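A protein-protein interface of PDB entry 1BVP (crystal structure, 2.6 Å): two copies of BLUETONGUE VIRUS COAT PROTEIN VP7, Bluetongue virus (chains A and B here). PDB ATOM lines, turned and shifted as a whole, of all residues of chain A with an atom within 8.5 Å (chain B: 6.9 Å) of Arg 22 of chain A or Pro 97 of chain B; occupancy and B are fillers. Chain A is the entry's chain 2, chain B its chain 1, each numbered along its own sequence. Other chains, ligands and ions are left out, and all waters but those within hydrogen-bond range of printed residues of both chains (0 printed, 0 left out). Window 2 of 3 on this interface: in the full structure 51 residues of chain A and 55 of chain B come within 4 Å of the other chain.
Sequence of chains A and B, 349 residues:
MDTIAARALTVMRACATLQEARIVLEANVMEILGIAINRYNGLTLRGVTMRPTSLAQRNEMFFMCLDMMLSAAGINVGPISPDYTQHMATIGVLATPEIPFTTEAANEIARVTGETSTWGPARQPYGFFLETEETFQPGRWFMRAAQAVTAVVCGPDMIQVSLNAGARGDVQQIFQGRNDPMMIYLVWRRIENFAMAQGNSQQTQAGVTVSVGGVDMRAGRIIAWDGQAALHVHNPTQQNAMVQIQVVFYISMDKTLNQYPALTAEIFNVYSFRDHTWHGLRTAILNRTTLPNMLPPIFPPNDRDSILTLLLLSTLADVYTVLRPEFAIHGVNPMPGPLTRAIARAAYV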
ATOM      1  N   LEU A  18     -34.457  -7.361  -9.265  1.00  0.00           N
ATOM      2  CA  LEU A  18     -33.741  -8.161 -10.254  1.00  0.00           C
ATOM      3  C   LEU A  18     -33.868  -7.652 -11.681  1.00  0.00           C
ATOM      4  O   LEU A  18     -34.211  -8.415 -12.597  1.00  0.00           O
ATOM      5  CB  LEU A  18     -34.223  -9.609 -10.160  1.00  0.00           C
ATOM      6  CG  LEU A  18     -33.665 -10.444  -8.985  1.00  0.00           C
ATOM      7  CD1 LEU A  18     -32.881  -9.627  -8.040  1.00  0.00           C
ATOM      8  CD2 LEU A  18     -34.760 -11.119  -8.230  1.00  0.00           C
ATOM      9  N   GLN A  19     -33.505  -6.388 -11.885  1.00  0.00           N
ATOM     10  CA  GLN A  19     -33.620  -5.758 -13.187  1.00  0.00           C
ATOM     11  C   GLN A  19     -32.720  -6.416 -14.217  1.00  0.00           C
ATOM     12  O   GLN A  19     -33.121  -6.689 -15.332  1.00  0.00           O
ATOM     13  CB  GLN A  19     -33.359  -4.228 -13.085  1.00  0.00           C
ATOM     14  CG  GLN A  19     -34.568  -3.285 -13.434  1.00  0.00           C
ATOM     15  CD  GLN A  19     -35.308  -2.682 -12.198  1.00  0.00           C
ATOM     16  OE1 GLN A  19     -35.971  -3.374 -11.425  1.00  0.00           O
ATOM     17  NE2 GLN A  19     -35.229  -1.378 -12.058  1.00  0.00           N
ATOM     18  N   GLU A  20     -31.532  -6.805 -13.820  1.00  0.00           N
ATOM     19  CA  GLU A  20     -30.649  -7.383 -14.808  1.00  0.00           C
ATOM     20  C   GLU A  20     -29.860  -8.581 -14.262  1.00  0.00           C
ATOM     21  O   GLU A  20     -30.011  -8.976 -13.090  1.00  0.00           O
ATOM     22  CB  GLU A  20     -29.797  -6.242 -15.374  1.00  0.00           C
ATOM     23  CG  GLU A  20     -28.611  -6.571 -16.188  1.00  0.00           C
ATOM     24  CD  GLU A  20     -27.525  -5.566 -15.897  1.00  0.00           C
ATOM     25  OE1 GLU A  20     -27.826  -4.353 -16.056  1.00  0.00           O
ATOM     26  OE2 GLU A  20     -26.414  -5.978 -15.446  1.00  0.00           O
ATOM     27  N   ALA A  21     -29.088  -9.202 -15.150  1.00  0.00           N
ATOM     28  CA  ALA A  21     -28.311 -10.390 -14.827  1.00  0.00           C
ATOM     29  C   ALA A  21     -27.087 -10.222 -13.915  1.00  0.00           C
ATOM     30  O   ALA A  21     -26.988 -10.898 -12.879  1.00  0.00           O
ATOM     31  CB  ALA A  21     -27.919 -11.106 -16.129  1.00  0.00           C
ATOM     32  N   ARG A  22     -26.180  -9.311 -14.267  1.00  0.00           N
ATOM     33  CA  ARG A  22     -24.953  -9.147 -13.481  1.00  0.00           C
ATOM     34  C   ARG A  22     -24.866  -8.090 -12.367  1.00  0.00           C
ATOM     35  O   ARG A  22     -23.845  -8.008 -11.679  1.00  0.00           O
ATOM     36  CB  ARG A  22     -23.723  -9.066 -14.414  1.00  0.00           C
ATOM     37  CG  ARG A  22     -23.712  -7.924 -15.458  1.00  0.00           C
ATOM     38  CD  ARG A  22     -22.366  -7.913 -16.206  1.00  0.00           C
ATOM     39  NE  ARG A  22     -21.242  -7.710 -15.277  1.00  0.00           N
ATOM     40  CZ  ARG A  22     -19.972  -8.058 -15.500  1.00  0.00           C
ATOM     41  NH1 ARG A  22     -19.621  -8.646 -16.640  1.00  0.00           N
ATOM     42  NH2 ARG A  22     -19.043  -7.806 -14.573  1.00  0.00           N
ATOM     43  N   ILE A  23     -25.927  -7.316 -12.166  1.00  0.00           N
ATOM     44  CA  ILE A  23     -25.951  -6.290 -11.129  1.00  0.00           C
ATOM     45  C   ILE A  23     -25.662  -6.824  -9.729  1.00  0.00           C
ATOM     46  O   ILE A  23     -25.795  -8.011  -9.481  1.00  0.00           O
ATOM     47  CB  ILE A  23     -27.303  -5.524 -11.154  1.00  0.00           C
ATOM     48  CG1 ILE A  23     -28.534  -6.461 -11.243  1.00  0.00           C
ATOM     49  CG2 ILE A  23     -27.312  -4.655 -12.395  1.00  0.00           C
ATOM     50  CD1 ILE A  23     -29.041  -7.127  -9.954  1.00  0.00           C
ATOM     51  N   VAL A  24     -25.216  -5.978  -8.814  1.00  0.00           N
ATOM     52  CA  VAL A  24     -24.963  -6.471  -7.472  1.00  0.00           C
ATOM     53  C   VAL A  24     -26.062  -6.026  -6.517  1.00  0.00           C
ATOM     54  O   VAL A  24     -26.430  -4.830  -6.428  1.00  0.00           O
ATOM     55  CB  VAL A  24     -23.563  -6.091  -6.920  1.00  0.00           C
ATOM     56  CG1 VAL A  24     -22.519  -6.228  -8.009  1.00  0.00           C
ATOM     57  CG2 VAL A  24     -23.568  -4.715  -6.277  1.00  0.00           C
ATOM     58  N   LEU A  25     -26.583  -7.010  -5.801  1.00  0.00           N
ATOM     59  CA  LEU A  25     -27.652  -6.765  -4.875  1.00  0.00           C
ATOM     60  C   LEU A  25     -27.259  -6.123  -3.575  1.00  0.00           C
ATOM     61  O   LEU A  25     -26.162  -6.315  -3.091  1.00  0.00           O
ATOM     62  CB  LEU A  25     -28.385  -8.069  -4.578  1.00  0.00           C
ATOM     63  CG  LEU A  25     -29.420  -8.499  -5.622  1.00  0.00           C
ATOM     64  CD1 LEU A  25     -29.916  -7.250  -6.406  1.00  0.00           C
ATOM     65  CD2 LEU A  25     -28.816  -9.560  -6.535  1.00  0.00           C
ATOM     66  N   ARG A  51     -31.147 -15.643  -8.911  1.00  0.00           N
ATOM     67  CA  ARG A  51     -30.827 -14.711  -9.982  1.00  0.00           C
ATOM     68  C   ARG A  51     -31.222 -15.356 -11.304  1.00  0.00           C
ATOM     69  O   ARG A  51     -30.431 -16.062 -11.932  1.00  0.00           O
ATOM     70  CB  ARG A  51     -29.342 -14.337  -9.983  1.00  0.00           C
ATOM     71  CG  ARG A  51     -29.009 -13.164 -10.931  1.00  0.00           C
ATOM     72  CD  ARG A  51     -29.101 -11.826 -10.208  1.00  0.00           C
ATOM     73  NE  ARG A  51     -28.368 -11.881  -8.928  1.00  0.00           N
ATOM     74  CZ  ARG A  51     -27.089 -11.532  -8.747  1.00  0.00           C
ATOM     75  NH1 ARG A  51     -26.364 -11.085  -9.769  1.00  0.00           N
ATOM     76  NH2 ARG A  51     -26.521 -11.644  -7.541  1.00  0.00           N
ATOM     77  N   PRO A  52     -32.474 -15.151 -11.727  1.00  0.00           N
ATOM     78  CA  PRO A  52     -33.037 -15.697 -12.966  1.00  0.00           C
ATOM     79  C   PRO A  52     -32.424 -15.102 -14.229  1.00  0.00           C
ATOM     80  O   PRO A  52     -32.214 -13.903 -14.306  1.00  0.00           O
ATOM     81  CB  PRO A  52     -34.501 -15.292 -12.865  1.00  0.00           C
ATOM     82  CG  PRO A  52     -34.706 -15.004 -11.385  1.00  0.00           C
ATOM     83  CD  PRO A  52     -33.464 -14.318 -11.025  1.00  0.00           C
ATOM     84  N   THR A  53     -32.142 -15.930 -15.228  1.00  0.00           N
ATOM     85  CA  THR A  53     -31.586 -15.443 -16.494  1.00  0.00           C
ATOM     86  C   THR A  53     -32.508 -15.854 -17.654  1.00  0.00           C
ATOM     87  O   THR A  53     -33.029 -14.999 -18.384  1.00  0.00           O
ATOM     88  CB  THR A  53     -30.109 -15.914 -16.709  1.00  0.00           C
ATOM     89  OG1 THR A  53     -29.986 -17.327 -16.470  1.00  0.00           O
ATOM     90  CG2 THR A  53     -29.207 -15.206 -15.720  1.00  0.00           C
ATOM     91  N   ARG B   7     -29.682   3.695  -9.921  1.00  0.00           N
ATOM     92  CA  ARG B   7     -28.432   4.070  -9.253  1.00  0.00           C
ATOM     93  C   ARG B   7     -28.335   5.545  -8.928  1.00  0.00           C
ATOM     94  O   ARG B   7     -27.987   5.910  -7.782  1.00  0.00           O
ATOM     95  CB  ARG B   7     -27.214   3.631 -10.041  1.00  0.00           C
ATOM     96  CG  ARG B   7     -27.091   2.137 -10.027  1.00  0.00           C
ATOM     97  CD  ARG B   7     -25.923   1.677 -10.848  1.00  0.00           C
ATOM     98  NE  ARG B   7     -25.909   0.219 -10.909  1.00  0.00           N
ATOM     99  CZ  ARG B   7     -25.966  -0.474 -12.040  1.00  0.00           C
ATOM    100  NH1 ARG B   7     -26.029   0.162 -13.194  1.00  0.00           N
ATOM    101  NH2 ARG B   7     -26.000  -1.799 -12.020  1.00  0.00           N
ATOM    102  N   ARG B  39     -15.942   5.318  -7.686  1.00  0.00           N
ATOM    103  CA  ARG B  39     -16.024   5.216  -9.156  1.00  0.00           C
ATOM    104  C   ARG B  39     -16.066   6.600  -9.786  1.00  0.00           C
ATOM    105  O   ARG B  39     -15.341   6.905 -10.727  1.00  0.00           O
ATOM    106  CB  ARG B  39     -17.264   4.469  -9.596  1.00  0.00           C
ATOM    107  CG  ARG B  39     -17.044   3.031  -9.910  1.00  0.00           C
ATOM    108  CD  ARG B  39     -16.028   2.846 -11.009  1.00  0.00           C
ATOM    109  NE  ARG B  39     -16.632   2.641 -12.320  1.00  0.00           N
ATOM    110  CZ  ARG B  39     -15.960   2.195 -13.380  1.00  0.00           C
ATOM    111  NH1 ARG B  39     -14.670   1.920 -13.276  1.00  0.00           N
ATOM    112  NH2 ARG B  39     -16.581   1.997 -14.538  1.00  0.00           N
ATOM    113  N   GLY B  92     -20.728   6.343 -17.506  1.00  0.00           N
ATOM    114  CA  GLY B  92     -19.911   5.159 -17.284  1.00  0.00           C
ATOM    115  C   GLY B  92     -19.929   4.798 -15.808  1.00  0.00           C
ATOM    116  O   GLY B  92     -19.930   3.637 -15.434  1.00  0.00           O
ATOM    117  N   VAL B  93     -19.919   5.804 -14.956  1.00  0.00           N
ATOM    118  CA  VAL B  93     -19.999   5.554 -13.538  1.00  0.00           C
ATOM    119  C   VAL B  93     -21.313   4.831 -13.221  1.00  0.00           C
ATOM    120  O   VAL B  93     -21.334   3.785 -12.585  1.00  0.00           O
ATOM    121  CB  VAL B  93     -20.015   6.869 -12.782  1.00  0.00           C
ATOM    122  CG1 VAL B  93     -20.249   6.603 -11.318  1.00  0.00           C
ATOM    123  CG2 VAL B  93     -18.716   7.660 -13.060  1.00  0.00           C
ATOM    124  N   LEU B  94     -22.418   5.398 -13.681  1.00  0.00           N
ATOM    125  CA  LEU B  94     -23.736   4.829 -13.427  1.00  0.00           C
ATOM    126  C   LEU B  94     -24.005   3.456 -14.055  1.00  0.00           C
ATOM    127  O   LEU B  94     -24.933   2.748 -13.635  1.00  0.00           O
ATOM    128  CB  LEU B  94     -24.796   5.808 -13.880  1.00  0.00           C
ATOM    129  CG  LEU B  94     -25.505   6.750 -12.927  1.00  0.00           C
ATOM    130  CD1 LEU B  94     -24.842   6.860 -11.598  1.00  0.00           C
ATOM    131  CD2 LEU B  94     -25.594   8.071 -13.618  1.00  0.00           C
ATOM    132  N   ALA B  95     -23.237   3.083 -15.077  1.00  0.00           N
ATOM    133  CA  ALA B  95     -23.429   1.770 -15.709  1.00  0.00           C
ATOM    134  C   ALA B  95     -22.569   0.670 -15.069  1.00  0.00           C
ATOM    135  O   ALA B  95     -22.559  -0.445 -15.553  1.00  0.00           O
ATOM    136  CB  ALA B  95     -23.157   1.852 -17.208  1.00  0.00           C
ATOM    137  N   THR B  96     -21.832   1.005 -14.006  1.00  0.00           N
ATOM    138  CA  THR B  96     -20.948   0.073 -13.284  1.00  0.00           C
ATOM    139  C   THR B  96     -21.810  -0.837 -12.409  1.00  0.00           C
ATOM    140  O   THR B  96     -22.342  -0.401 -11.387  1.00  0.00           O
ATOM    141  CB  THR B  96     -19.974   0.859 -12.326  1.00  0.00           C
ATOM    142  OG1 THR B  96     -19.134   1.736 -13.085  1.00  0.00           O
ATOM    143  CG2 THR B  96     -19.103  -0.088 -11.497  1.00  0.00           C
ATOM    144  N   PRO B  97     -21.851  -2.137 -12.722  1.00  0.00           N
ATOM    145  CA  PRO B  97     -22.654  -3.093 -11.949  1.00  0.00           C
ATOM    146  C   PRO B  97     -22.301  -3.252 -10.498  1.00  0.00           C
ATOM    147  O   PRO B  97     -23.037  -3.862  -9.746  1.00  0.00           O
ATOM    148  CB  PRO B  97     -22.496  -4.403 -12.722  1.00  0.00           C
ATOM    149  CG  PRO B  97     -21.197  -4.242 -13.404  1.00  0.00           C
ATOM    150  CD  PRO B  97     -21.177  -2.803 -13.847  1.00  0.00           C
ATOM    151  N   GLU B  98     -21.204  -2.661 -10.072  1.00  0.00           N
ATOM    152  CA  GLU B  98     -20.824  -2.795  -8.676  1.00  0.00           C
ATOM    153  C   GLU B  98     -21.482  -1.781  -7.775  1.00  0.00           C
ATOM    154  O   GLU B  98     -21.436  -1.953  -6.551  1.00  0.00           O
ATOM    155  CB  GLU B  98     -19.298  -2.802  -8.487  1.00  0.00           C
ATOM    156  CG  GLU B  98     -18.602  -4.108  -8.918  1.00  0.00           C
ATOM    157  CD  GLU B  98     -18.366  -4.213 -10.431  1.00  0.00           C
ATOM    158  OE1 GLU B  98     -17.940  -3.199 -11.070  1.00  0.00           O
ATOM    159  OE2 GLU B  98     -18.584  -5.327 -10.974  1.00  0.00           O
ATOM    160  N   ILE B  99     -22.032  -0.701  -8.339  1.00  0.00           N
ATOM    161  CA  ILE B  99     -22.732   0.288  -7.502  1.00  0.00           C
ATOM    162  C   ILE B  99     -24.129  -0.282  -7.295  1.00  0.00           C
ATOM    163  O   ILE B  99     -24.872  -0.514  -8.254  1.00  0.00           O
ATOM    164  CB  ILE B  99     -22.889   1.647  -8.154  1.00  0.00           C
ATOM    165  CG1 ILE B  99     -21.526   2.194  -8.582  1.00  0.00           C
ATOM    166  CG2 ILE B  99     -23.592   2.585  -7.168  1.00  0.00           C
ATOM    167  CD1 ILE B  99     -21.593   3.599  -9.090  1.00  0.00           C
ATOM    168  N   PRO B 100     -24.486  -0.567  -6.043  1.00  0.00           N
ATOM    169  CA  PRO B 100     -25.820  -1.129  -5.799  1.00  0.00           C
ATOM    170  C   PRO B 100     -26.943  -0.064  -5.760  1.00  0.00           C
ATOM    171  O   PRO B 100     -26.689   1.132  -5.589  1.00  0.00           O
ATOM    172  CB  PRO B 100     -25.635  -1.836  -4.448  1.00  0.00           C
ATOM    173  CG  PRO B 100     -24.709  -0.864  -3.724  1.00  0.00           C
ATOM    174  CD  PRO B 100     -23.743  -0.334  -4.784  1.00  0.00           C
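Among the printed residues, pairs that only touch across the chains: Arg 22 of chain A with Pro 97 of chain B, Ile 23 of chain A with Arg 7 of chain B, Ile 23 of chain A with Pro 97 of chain B, Val 24 of chain A with Glu 98 of chain B and Val 24 of chain A with Pro 100 of chain B.
The backbone carbonyl oxygen of Pro 97 of chain B lies close to the backbone NH of Val 24 of chain A (3.2 Å).
Of chain B, only Pro 97 comes within 4 Å of Arg 22 of chain A. Of the printed residues of chain B, Ile 23 of chain A touches Arg 7 and Pro 97. Pro 52 of chain A touches none of the printed residues of chain B. Pro 97 of chain B touches just these residues of chain A: Arg 22 (3.9 Å), Ile 23 (3.96 Å) and Val 24 (3.0 Å). Of chain A, only Val 24 (3.5 Å) comes within 4 Å of Glu 98 of chain B. Of the printed residues of chain A, Pro 100 of chain B touches Val 24 (3.7 Å). The nearest residue of chain A that does not touch Pro 97 of chain B is Glu 20 of chain A (5.0 Å). The nearest printed residue of chain A that does not touch Pro 100 of chain B is Leu 25 of chain A (4.7 Å).
No position is printed for both chains. Of the 6 pairs that touch across the chains among the printed residues, none has its exchanged pair printed and touching as well.
The backbone carbonyl oxygen of Leu 94 of chain B is in hydrogen-bond range of the guanidinium group of Arg 7 of chain B, 2.8 Å away. The backbone carbonyl oxygen (O) of Ile 99 of chain B lies within hydrogen-bond range of the guanidinium group (NE) of Arg 7 of chain B (2.9 Å). O of Ile 23 of chain A lies within hydrogen-bond range of NH1 of Arg 51 of chain A (3.1 Å).
Of the 11 printed residues of chain A, 3 touch a printed residue of chain B. Hydrophobic or aromatic side chains of chain A within 4 Å of the printed part of chain B: Ile 23 and Val 24. Of the 11 printed residues of chain B, 4 touch a printed residue of chain A. Hydrophobic or aromatic side chains of chain B that line the printed part of chain A: Pro 97 and Pro 100. Among the printed residues, 6 pairs touch across the chains. Among the printed residues, no Asp or Glu carboxylate lies within 4 Å of a Lys or Arg side-chain nitrogen of the other chain.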
